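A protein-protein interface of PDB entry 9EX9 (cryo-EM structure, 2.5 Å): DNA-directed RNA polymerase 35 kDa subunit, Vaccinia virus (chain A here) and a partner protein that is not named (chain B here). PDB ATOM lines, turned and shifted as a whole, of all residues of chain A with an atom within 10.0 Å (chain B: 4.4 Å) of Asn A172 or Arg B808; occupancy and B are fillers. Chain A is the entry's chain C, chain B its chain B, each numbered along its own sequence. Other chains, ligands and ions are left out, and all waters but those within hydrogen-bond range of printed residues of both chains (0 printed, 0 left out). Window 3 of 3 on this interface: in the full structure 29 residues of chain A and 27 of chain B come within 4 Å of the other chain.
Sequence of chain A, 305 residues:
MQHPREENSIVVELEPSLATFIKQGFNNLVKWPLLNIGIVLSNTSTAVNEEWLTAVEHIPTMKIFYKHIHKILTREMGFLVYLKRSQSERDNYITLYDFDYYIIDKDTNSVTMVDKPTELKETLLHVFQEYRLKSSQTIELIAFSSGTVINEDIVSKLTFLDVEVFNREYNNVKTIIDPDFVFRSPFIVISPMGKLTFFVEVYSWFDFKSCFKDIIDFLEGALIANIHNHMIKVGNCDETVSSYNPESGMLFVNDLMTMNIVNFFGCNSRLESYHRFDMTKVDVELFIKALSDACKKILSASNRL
Asn B810 touches Asn A49.
ND2 of Asn B810 touches OE1 of Glu A169, 3.98 Å away.
Asn A172 touches Leu B809 (ND2 to O, 3.7 Å).
CB of Asn A172 touches O of Asn B810 (3.7 Å).
OD1 of Asn A172 touches CB of Ala B811, 3.7 Å away.
Asn A172 touches Phe B812 (O to CD1, 3.6 Å).
CD1 of Ile A176 touches CZ of Phe B812, at 3.5 Å.
The guanidinium group of Arg B808 sits at hydrogen-bond distance from the side-chain amide oxygen of Asn A172.
N of Arg B808 sits at hydrogen-bond distance from O of Lys B800, 3.1 Å away.
The side-chain amino group (NZ) of Lys B800 sits at hydrogen-bond distance from the backbone carbonyl oxygen (O) of Phe B812 (2.6 Å).
The side-chain carboxylate (OE2) of Glu B802 lies within salt-bridge range of the guanidinium group (NH1) of Arg B808 (3.9 Å).
The backbone NH (N) of Asn B810 lies within hydrogen-bond range of the backbone carbonyl oxygen (O) of Val B854 (3.0 Å).
The backbone carbonyl oxygen (O) of Ala B811 is in hydrogen-bond range of the backbone NH (N) of Val B854 (3.0 Å).
NH2 of Arg A168 lies within salt-bridge range of OE2 of Glu A169 (3.3 Å).
Hydrophobic or aromatic side chains of chain A within 4 Å of the printed part of chain B: Ile A176.
Of the 11 printed residues of chain B, 5 touch a printed residue of chain A.
Printed residues of chain B that touch a printed residue of chain A: Arg B808, Leu B809, Asn B810, Ala B811 and Phe B812.
Among the printed residues, 8 pairs touch across the chains.
Among the printed residues, no Asp or Glu carboxylate lies within 4 Å of a Lys or Arg side-chain nitrogen of the other chain.
Printed residues of chain B within 4 Å of Asn A49: Asn B810 (3.996 Å).
Arg A168 touches none of the printed residues of chain B.
Printed residues of chain B within 4 Å of Glu A169: Asn B810 (3.98 Å).
Asn A172 touches five residues of chain B.
Of chain A, only Asn A172 comes within 4 Å of Arg B808.
Of the printed residues of chain A, Asn B810 touches Asn A49, Glu A169 and Asn A172.
Of chain A, only Asn A172 (3.7 Å) comes within 4 Å of Ala B811.
Printed residues of chain A within 4 Å of Phe B812: Asn A172 (3.6 Å) and Ile A176 (3.5 Å).
No residue of chain A comes within 4 Å of Val B854.
The nearest printed residue of chain B that does not touch Asn A172 is Lys B800 (6.3 Å).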
ATOM      1  N   GLY A  38     -12.816  10.288  23.013  1.00  0.00           N
ATOM      2  CA  GLY A  38     -12.766  11.190  21.870  1.00  0.00           C
ATOM      3  C   GLY A  38     -11.358  11.422  21.361  1.00  0.00           C
ATOM      4  O   GLY A  38     -10.441  11.659  22.146  1.00  0.00           O
ATOM      5  N   ILE A  39     -11.200  11.368  20.039  1.00  0.00           N
ATOM      6  CA  ILE A  39      -9.926  11.613  19.373  1.00  0.00           C
ATOM      7  C   ILE A  39     -10.153  12.619  18.254  1.00  0.00           C
ATOM      8  O   ILE A  39     -11.031  12.424  17.406  1.00  0.00           O
ATOM      9  CB  ILE A  39      -9.314  10.316  18.810  1.00  0.00           C
ATOM     10  CG1 ILE A  39      -9.133   9.276  19.918  1.00  0.00           C
ATOM     11  CG2 ILE A  39      -7.984  10.600  18.147  1.00  0.00           C
ATOM     12  CD1 ILE A  39     -10.280   8.306  20.039  1.00  0.00           C
ATOM     13  N   VAL A  40      -9.354  13.684  18.242  1.00  0.00           N
ATOM     14  CA  VAL A  40      -9.397  14.699  17.194  1.00  0.00           C
ATOM     15  C   VAL A  40      -8.249  14.425  16.236  1.00  0.00           C
ATOM     16  O   VAL A  40      -7.077  14.505  16.622  1.00  0.00           O
ATOM     17  CB  VAL A  40      -9.299  16.119  17.775  1.00  0.00           C
ATOM     18  CG1 VAL A  40      -9.209  17.138  16.663  1.00  0.00           C
ATOM     19  CG2 VAL A  40     -10.490  16.421  18.652  1.00  0.00           C
ATOM     20  N   LEU A  41      -8.573  14.097  14.988  1.00  0.00           N
ATOM     21  CA  LEU A  41      -7.545  13.743  14.022  1.00  0.00           C
ATOM     22  C   LEU A  41      -6.994  14.951  13.277  1.00  0.00           C
ATOM     23  O   LEU A  41      -5.806  14.972  12.942  1.00  0.00           O
ATOM     24  CB  LEU A  41      -8.103  12.735  13.019  1.00  0.00           C
ATOM     25  CG  LEU A  41      -8.750  11.503  13.645  1.00  0.00           C
ATOM     26  CD1 LEU A  41      -9.390  10.648  12.590  1.00  0.00           C
ATOM     27  CD2 LEU A  41      -7.735  10.700  14.413  1.00  0.00           C
ATOM     28  N   ASN A  49      -9.010  21.804  20.603  1.00  0.00           N
ATOM     29  CA  ASN A  49      -9.494  20.426  20.669  1.00  0.00           C
ATOM     30  C   ASN A  49     -10.472  20.236  21.819  1.00  0.00           C
ATOM     31  O   ASN A  49     -11.481  19.531  21.681  1.00  0.00           O
ATOM     32  CB  ASN A  49      -8.318  19.463  20.834  1.00  0.00           C
ATOM     33  CG  ASN A  49      -7.386  19.458  19.646  1.00  0.00           C
ATOM     34  OD1 ASN A  49      -7.591  20.181  18.676  1.00  0.00           O
ATOM     35  ND2 ASN A  49      -6.346  18.641  19.722  1.00  0.00           N
ATOM     36  N   LEU A  53     -14.215  18.432  21.883  1.00  0.00           N
ATOM     37  CA  LEU A  53     -14.390  17.160  22.573  1.00  0.00           C
ATOM     38  C   LEU A  53     -15.480  17.250  23.632  1.00  0.00           C
ATOM     39  O   LEU A  53     -16.351  16.377  23.718  1.00  0.00           O
ATOM     40  CB  LEU A  53     -13.066  16.716  23.195  1.00  0.00           C
ATOM     41  CG  LEU A  53     -11.975  16.274  22.219  1.00  0.00           C
ATOM     42  CD1 LEU A  53     -10.756  15.803  22.973  1.00  0.00           C
ATOM     43  CD2 LEU A  53     -12.476  15.182  21.297  1.00  0.00           C
ATOM     44  N   GLU A 164      -3.188   4.976  10.265  1.00  0.00           N
ATOM     45  CA  GLU A 164      -1.961   5.503  10.856  1.00  0.00           C
ATOM     46  C   GLU A 164      -2.237   6.768  11.660  1.00  0.00           C
ATOM     47  O   GLU A 164      -1.722   6.943  12.774  1.00  0.00           O
ATOM     48  CB  GLU A 164      -0.933   5.776   9.761  1.00  0.00           C
ATOM     49  CG  GLU A 164       0.358   6.397  10.265  1.00  0.00           C
ATOM     50  CD  GLU A 164       1.276   6.815   9.140  1.00  0.00           C
ATOM     51  OE1 GLU A 164       1.070   6.349   8.001  1.00  0.00           O
ATOM     52  OE2 GLU A 164       2.200   7.615   9.394  1.00  0.00           O
ATOM     53  N   VAL A 165      -3.046   7.669  11.102  1.00  0.00           N
ATOM     54  CA  VAL A 165      -3.379   8.902  11.805  1.00  0.00           C
ATOM     55  C   VAL A 165      -4.104   8.583  13.101  1.00  0.00           C
ATOM     56  O   VAL A 165      -3.836   9.186  14.150  1.00  0.00           O
ATOM     57  CB  VAL A 165      -4.220   9.818  10.900  1.00  0.00           C
ATOM     58  CG1 VAL A 165      -4.625  11.065  11.650  1.00  0.00           C
ATOM     59  CG2 VAL A 165      -3.448  10.183   9.650  1.00  0.00           C
ATOM     60  N   PHE A 166      -5.043   7.636  13.047  1.00  0.00           N
ATOM     61  CA  PHE A 166      -5.770   7.258  14.250  1.00  0.00           C
ATOM     62  C   PHE A 166      -4.828   6.696  15.302  1.00  0.00           C
ATOM     63  O   PHE A 166      -4.936   7.036  16.483  1.00  0.00           O
ATOM     64  CB  PHE A 166      -6.859   6.239  13.919  1.00  0.00           C
ATOM     65  CG  PHE A 166      -7.692   5.853  15.106  1.00  0.00           C
ATOM     66  CD1 PHE A 166      -8.853   6.537  15.405  1.00  0.00           C
ATOM     67  CD2 PHE A 166      -7.304   4.820  15.936  1.00  0.00           C
ATOM     68  CE1 PHE A 166      -9.608   6.193  16.499  1.00  0.00           C
ATOM     69  CE2 PHE A 166      -8.059   4.477  17.029  1.00  0.00           C
ATOM     70  CZ  PHE A 166      -9.212   5.165  17.308  1.00  0.00           C
ATOM     71  N   ASN A 167      -3.901   5.830  14.899  1.00  0.00           N
ATOM     72  CA  ASN A 167      -2.972   5.253  15.862  1.00  0.00           C
ATOM     73  C   ASN A 167      -2.147   6.341  16.529  1.00  0.00           C
ATOM     74  O   ASN A 167      -2.019   6.376  17.760  1.00  0.00           O
ATOM     75  CB  ASN A 167      -2.065   4.237  15.174  1.00  0.00           C
ATOM     76  CG  ASN A 167      -2.805   2.998  14.739  1.00  0.00           C
ATOM     77  OD1 ASN A 167      -2.846   2.669  13.557  1.00  0.00           O
ATOM     78  ND2 ASN A 167      -3.392   2.297  15.695  1.00  0.00           N
ATOM     79  N   ARG A 168      -1.599   7.259  15.732  1.00  0.00           N
ATOM     80  CA  ARG A 168      -0.774   8.321  16.298  1.00  0.00           C
ATOM     81  C   ARG A 168      -1.571   9.167  17.284  1.00  0.00           C
ATOM     82  O   ARG A 168      -1.149   9.383  18.429  1.00  0.00           O
ATOM     83  CB  ARG A 168      -0.207   9.190  15.178  1.00  0.00           C
ATOM     84  CG  ARG A 168       0.793  10.222  15.652  1.00  0.00           C
ATOM     85  CD  ARG A 168       1.357  11.046  14.509  1.00  0.00           C
ATOM     86  NE  ARG A 168       0.355  11.918  13.908  1.00  0.00           N
ATOM     87  CZ  ARG A 168      -0.181  11.755  12.705  1.00  0.00           C
ATOM     88  NH1 ARG A 168       0.176  10.757  11.913  1.00  0.00           N
ATOM     89  NH2 ARG A 168      -1.097  12.622  12.281  1.00  0.00           N
ATOM     90  N   GLU A 169      -2.745   9.638  16.866  1.00  0.00           N
ATOM     91  CA  GLU A 169      -3.497  10.552  17.717  1.00  0.00           C
ATOM     92  C   GLU A 169      -4.027   9.851  18.962  1.00  0.00           C
ATOM     93  O   GLU A 169      -4.027  10.434  20.053  1.00  0.00           O
ATOM     94  CB  GLU A 169      -4.628  11.189  16.917  1.00  0.00           C
ATOM     95  CG  GLU A 169      -4.141  11.977  15.707  1.00  0.00           C
ATOM     96  CD  GLU A 169      -3.180  13.100  16.070  1.00  0.00           C
ATOM     97  OE1 GLU A 169      -3.123  13.488  17.252  1.00  0.00           O
ATOM     98  OE2 GLU A 169      -2.477  13.599  15.169  1.00  0.00           O
ATOM     99  N   TYR A 170      -4.476   8.600  18.833  1.00  0.00           N
ATOM    100  CA  TYR A 170      -4.924   7.871  20.011  1.00  0.00           C
ATOM    101  C   TYR A 170      -3.784   7.671  20.995  1.00  0.00           C
ATOM    102  O   TYR A 170      -3.965   7.849  22.204  1.00  0.00           O
ATOM    103  CB  TYR A 170      -5.524   6.525  19.615  1.00  0.00           C
ATOM    104  CG  TYR A 170      -5.998   5.738  20.811  1.00  0.00           C
ATOM    105  CD1 TYR A 170      -7.081   6.168  21.556  1.00  0.00           C
ATOM    106  CD2 TYR A 170      -5.356   4.579  21.207  1.00  0.00           C
ATOM    107  CE1 TYR A 170      -7.513   5.465  22.654  1.00  0.00           C
ATOM    108  CE2 TYR A 170      -5.783   3.871  22.305  1.00  0.00           C
ATOM    109  CZ  TYR A 170      -6.862   4.318  23.024  1.00  0.00           C
ATOM    110  OH  TYR A 170      -7.296   3.617  24.120  1.00  0.00           O
ATOM    111  N   ASN A 171      -2.597   7.310  20.503  1.00  0.00           N
ATOM    112  CA  ASN A 171      -1.455   7.211  21.403  1.00  0.00           C
ATOM    113  C   ASN A 171      -1.155   8.553  22.051  1.00  0.00           C
ATOM    114  O   ASN A 171      -0.603   8.600  23.154  1.00  0.00           O
ATOM    115  CB  ASN A 171      -0.232   6.697  20.649  1.00  0.00           C
ATOM    116  CG  ASN A 171      -0.514   5.414  19.900  1.00  0.00           C
ATOM    117  OD1 ASN A 171      -1.441   4.680  20.231  1.00  0.00           O
ATOM    118  ND2 ASN A 171       0.283   5.138  18.879  1.00  0.00           N
ATOM    119  N   ASN A 172      -1.506   9.651  21.382  1.00  0.00           N
ATOM    120  CA  ASN A 172      -1.309  10.963  21.993  1.00  0.00           C
ATOM    121  C   ASN A 172      -2.303  11.223  23.123  1.00  0.00           C
ATOM    122  O   ASN A 172      -1.921  11.738  24.179  1.00  0.00           O
ATOM    123  CB  ASN A 172      -1.413  12.060  20.936  1.00  0.00           C
ATOM    124  CG  ASN A 172      -0.096  12.328  20.242  1.00  0.00           C
ATOM    125  OD1 ASN A 172       0.972  12.093  20.801  1.00  0.00           O
ATOM    126  ND2 ASN A 172      -0.167  12.832  19.020  1.00  0.00           N
ATOM    127  N   VAL A 173      -3.580  10.879  22.933  1.00  0.00           N
ATOM    128  CA  VAL A 173      -4.619  11.284  23.885  1.00  0.00           C
ATOM    129  C   VAL A 173      -4.917  10.244  24.958  1.00  0.00           C
ATOM    130  O   VAL A 173      -5.544  10.590  25.970  1.00  0.00           O
ATOM    131  CB  VAL A 173      -5.946  11.637  23.174  1.00  0.00           C
ATOM    132  CG1 VAL A 173      -5.731  12.711  22.135  1.00  0.00           C
ATOM    133  CG2 VAL A 173      -6.565  10.411  22.545  1.00  0.00           C
ATOM    134  N   LYS A 174      -4.487   8.993  24.787  1.00  0.00           N
ATOM    135  CA  LYS A 174      -5.009   7.919  25.631  1.00  0.00           C
ATOM    136  C   LYS A 174      -4.763   8.166  27.113  1.00  0.00           C
ATOM    137  O   LYS A 174      -5.513   7.659  27.952  1.00  0.00           O
ATOM    138  CB  LYS A 174      -4.397   6.580  25.225  1.00  0.00           C
ATOM    139  CG  LYS A 174      -2.894   6.493  25.420  1.00  0.00           C
ATOM    140  CD  LYS A 174      -2.403   5.058  25.391  1.00  0.00           C
ATOM    141  CE  LYS A 174      -2.801   4.355  24.112  1.00  0.00           C
ATOM    142  NZ  LYS A 174      -2.137   3.032  23.978  1.00  0.00           N
ATOM    143  N   THR A 175      -3.730   8.928  27.465  1.00  0.00           N
ATOM    144  CA  THR A 175      -3.344   9.038  28.867  1.00  0.00           C
ATOM    145  C   THR A 175      -4.255   9.947  29.680  1.00  0.00           C
ATOM    146  O   THR A 175      -4.189   9.912  30.912  1.00  0.00           O
ATOM    147  CB  THR A 175      -1.908   9.547  28.985  1.00  0.00           C
ATOM    148  OG1 THR A 175      -1.775  10.787  28.285  1.00  0.00           O
ATOM    149  CG2 THR A 175      -0.941   8.533  28.410  1.00  0.00           C
ATOM    150  N   ILE A 176      -5.093  10.764  29.038  1.00  0.00           N
ATOM    151  CA  ILE A 176      -5.993  11.654  29.768  1.00  0.00           C
ATOM    152  C   ILE A 176      -7.432  11.167  29.770  1.00  0.00           C
ATOM    153  O   ILE A 176      -8.238  11.672  30.566  1.00  0.00           O
ATOM    154  CB  ILE A 176      -5.949  13.092  29.210  1.00  0.00           C
ATOM    155  CG1 ILE A 176      -6.315  13.110  27.728  1.00  0.00           C
ATOM    156  CG2 ILE A 176      -4.576  13.695  29.430  1.00  0.00           C
ATOM    157  CD1 ILE A 176      -6.856  14.431  27.266  1.00  0.00           C
ATOM    158  N   ILE A 177      -7.787  10.217  28.909  1.00  0.00           N
ATOM    159  CA  ILE A 177      -9.125   9.644  28.946  1.00  0.00           C
ATOM    160  C   ILE A 177      -9.313   8.919  30.270  1.00  0.00           C
ATOM    161  O   ILE A 177      -8.501   8.066  30.649  1.00  0.00           O
ATOM    162  CB  ILE A 177      -9.333   8.700  27.754  1.00  0.00           C
ATOM    163  CG1 ILE A 177      -9.240   9.481  26.446  1.00  0.00           C
ATOM    164  CG2 ILE A 177     -10.675   7.993  27.861  1.00  0.00           C
ATOM    165  CD1 ILE A 177      -9.235   8.612  25.220  1.00  0.00           C
ATOM    166  N   SER B 799      11.080  10.890  25.411  1.00  0.00           N
ATOM    167  CA  SER B 799      10.042  10.027  24.861  1.00  0.00           C
ATOM    168  C   SER B 799       9.124  10.779  23.907  1.00  0.00           C
ATOM    169  O   SER B 799       8.583  10.180  22.971  1.00  0.00           O
ATOM    170  CB  SER B 799       9.229   9.407  25.995  1.00  0.00           C
ATOM    171  OG  SER B 799       8.746  10.406  26.873  1.00  0.00           O
ATOM    172  N   LYS B 800       8.943  12.080  24.115  1.00  0.00           N
ATOM    173  CA  LYS B 800       8.012  12.878  23.330  1.00  0.00           C
ATOM    174  C   LYS B 800       8.684  13.594  22.166  1.00  0.00           C
ATOM    175  O   LYS B 800       8.052  14.441  21.531  1.00  0.00           O
ATOM    176  CB  LYS B 800       7.313  13.902  24.225  1.00  0.00           C
ATOM    177  CG  LYS B 800       6.707  13.327  25.495  1.00  0.00           C
ATOM    178  CD  LYS B 800       5.507  12.453  25.205  1.00  0.00           C
ATOM    179  CE  LYS B 800       5.091  11.667  26.434  1.00  0.00           C
ATOM    180  NZ  LYS B 800       4.855  12.542  27.611  1.00  0.00           N
ATOM    181  N   GLU B 802      10.470  14.012  18.445  1.00  0.00           N
ATOM    182  CA  GLU B 802      10.460  13.481  17.095  1.00  0.00           C
ATOM    183  C   GLU B 802      11.893  13.261  16.613  1.00  0.00           C
ATOM    184  O   GLU B 802      12.864  13.506  17.331  1.00  0.00           O
ATOM    185  CB  GLU B 802       9.709  14.425  16.163  1.00  0.00           C
ATOM    186  CG  GLU B 802       8.206  14.351  16.292  1.00  0.00           C
ATOM    187  CD  GLU B 802       7.639  13.073  15.715  1.00  0.00           C
ATOM    188  OE1 GLU B 802       8.428  12.243  15.222  1.00  0.00           O
ATOM    189  OE2 GLU B 802       6.404  12.897  15.751  1.00  0.00           O
ATOM    190  N   LEU B 806      12.687  17.868  18.197  1.00  0.00           N
ATOM    191  CA  LEU B 806      11.661  18.763  18.705  1.00  0.00           C
ATOM    192  C   LEU B 806      10.455  17.956  19.160  1.00  0.00           C
ATOM    193  O   LEU B 806      10.151  16.896  18.606  1.00  0.00           O
ATOM    194  CB  LEU B 806      11.230  19.776  17.640  1.00  0.00           C
ATOM    195  CG  LEU B 806      12.303  20.748  17.155  1.00  0.00           C
ATOM    196  CD1 LEU B 806      11.793  21.543  15.976  1.00  0.00           C
ATOM    197  CD2 LEU B 806      12.732  21.673  18.271  1.00  0.00           C
ATOM    198  N   VAL B 807       9.765  18.475  20.177  1.00  0.00           N
ATOM    199  CA  VAL B 807       8.612  17.778  20.725  1.00  0.00           C
ATOM    200  C   VAL B 807       7.523  17.644  19.666  1.00  0.00           C
ATOM    201  O   VAL B 807       7.426  18.445  18.730  1.00  0.00           O
ATOM    202  CB  VAL B 807       8.087  18.513  21.970  1.00  0.00           C
ATOM    203  CG1 VAL B 807       7.620  19.906  21.609  1.00  0.00           C
ATOM    204  CG2 VAL B 807       6.971  17.727  22.620  1.00  0.00           C
ATOM    205  N   ARG B 808       6.696  16.616  19.818  1.00  0.00           N
ATOM    206  CA  ARG B 808       5.667  16.304  18.840  1.00  0.00           C
ATOM    207  C   ARG B 808       4.391  17.094  19.116  1.00  0.00           C
ATOM    208  O   ARG B 808       4.026  17.346  20.266  1.00  0.00           O
ATOM    209  CB  ARG B 808       5.372  14.805  18.861  1.00  0.00           C
ATOM    210  CG  ARG B 808       4.253  14.368  17.941  1.00  0.00           C
ATOM    211  CD  ARG B 808       4.076  12.859  17.955  1.00  0.00           C
ATOM    212  NE  ARG B 808       3.982  12.322  19.308  1.00  0.00           N
ATOM    213  CZ  ARG B 808       5.004  11.844  20.005  1.00  0.00           C
ATOM    214  NH1 ARG B 808       6.232  11.824  19.514  1.00  0.00           N
ATOM    215  NH2 ARG B 808       4.789  11.373  21.230  1.00  0.00           N
ATOM    216  N   LEU B 809       3.712  17.486  18.042  1.00  0.00           N
ATOM    217  CA  LEU B 809       2.463  18.222  18.178  1.00  0.00           C
ATOM    218  C   LEU B 809       1.390  17.355  18.822  1.00  0.00           C
ATOM    219  O   LEU B 809       1.272  16.163  18.527  1.00  0.00           O
ATOM    220  CB  LEU B 809       1.971  18.704  16.813  1.00  0.00           C
ATOM    221  CG  LEU B 809       2.670  19.892  16.153  1.00  0.00           C
ATOM    222  CD1 LEU B 809       1.979  20.219  14.850  1.00  0.00           C
ATOM    223  CD2 LEU B 809       2.675  21.104  17.060  1.00  0.00           C
ATOM    224  N   ASN B 810       0.597  17.967  19.699  1.00  0.00           N
ATOM    225  CA  ASN B 810      -0.570  17.369  20.339  1.00  0.00           C
ATOM    226  C   ASN B 810      -0.217  16.325  21.386  1.00  0.00           C
ATOM    227  O   ASN B 810      -1.116  15.657  21.899  1.00  0.00           O
ATOM    228  CB  ASN B 810      -1.516  16.740  19.312  1.00  0.00           C
ATOM    229  CG  ASN B 810      -2.158  17.766  18.411  1.00  0.00           C
ATOM    230  OD1 ASN B 810      -2.457  18.877  18.835  1.00  0.00           O
ATOM    231  ND2 ASN B 810      -2.377  17.399  17.159  1.00  0.00           N
ATOM    232  N   ALA B 811       1.054  16.164  21.724  1.00  0.00           N
ATOM    233  CA  ALA B 811       1.453  15.242  22.773  1.00  0.00           C
ATOM    234  C   ALA B 811       1.323  15.907  24.136  1.00  0.00           C
ATOM    235  O   ALA B 811       1.309  17.131  24.255  1.00  0.00           O
ATOM    236  CB  ALA B 811       2.889  14.771  22.563  1.00  0.00           C
ATOM    237  N   PHE B 812       1.231  15.084  25.172  1.00  0.00           N
ATOM    238  CA  PHE B 812       1.091  15.569  26.537  1.00  0.00           C
ATOM    239  C   PHE B 812       2.415  15.428  27.276  1.00  0.00           C
ATOM    240  O   PHE B 812       2.999  14.341  27.314  1.00  0.00           O
ATOM    241  CB  PHE B 812      -0.011  14.815  27.278  1.00  0.00           C
ATOM    242  CG  PHE B 812      -1.390  15.312  26.970  1.00  0.00           C
ATOM    243  CD1 PHE B 812      -2.042  14.916  25.820  1.00  0.00           C
ATOM    244  CD2 PHE B 812      -2.033  16.176  27.831  1.00  0.00           C
ATOM    245  CE1 PHE B 812      -3.305  15.372  25.537  1.00  0.00           C
ATOM    246  CE2 PHE B 812      -3.299  16.634  27.549  1.00  0.00           C
ATOM    247  CZ  PHE B 812      -3.933  16.230  26.401  1.00  0.00           C
ATOM    248  N   VAL B 854       0.763  20.076  23.726  1.00  0.00           N
ATOM    249  CA  VAL B 854       1.605  20.957  22.925  1.00  0.00           C
ATOM    250  C   VAL B 854       0.759  21.500  21.782  1.00  0.00           C
ATOM    251  O   VAL B 854       0.415  20.771  20.850  1.00  0.00           O
ATOM    252  CB  VAL B 854       2.845  20.227  22.403  1.00  0.00           C
ATOM    253  CG1 VAL B 854       3.596  21.098  21.423  1.00  0.00           C
ATOM    254  CG2 VAL B 854       3.742  19.835  23.556  1.00  0.00           C
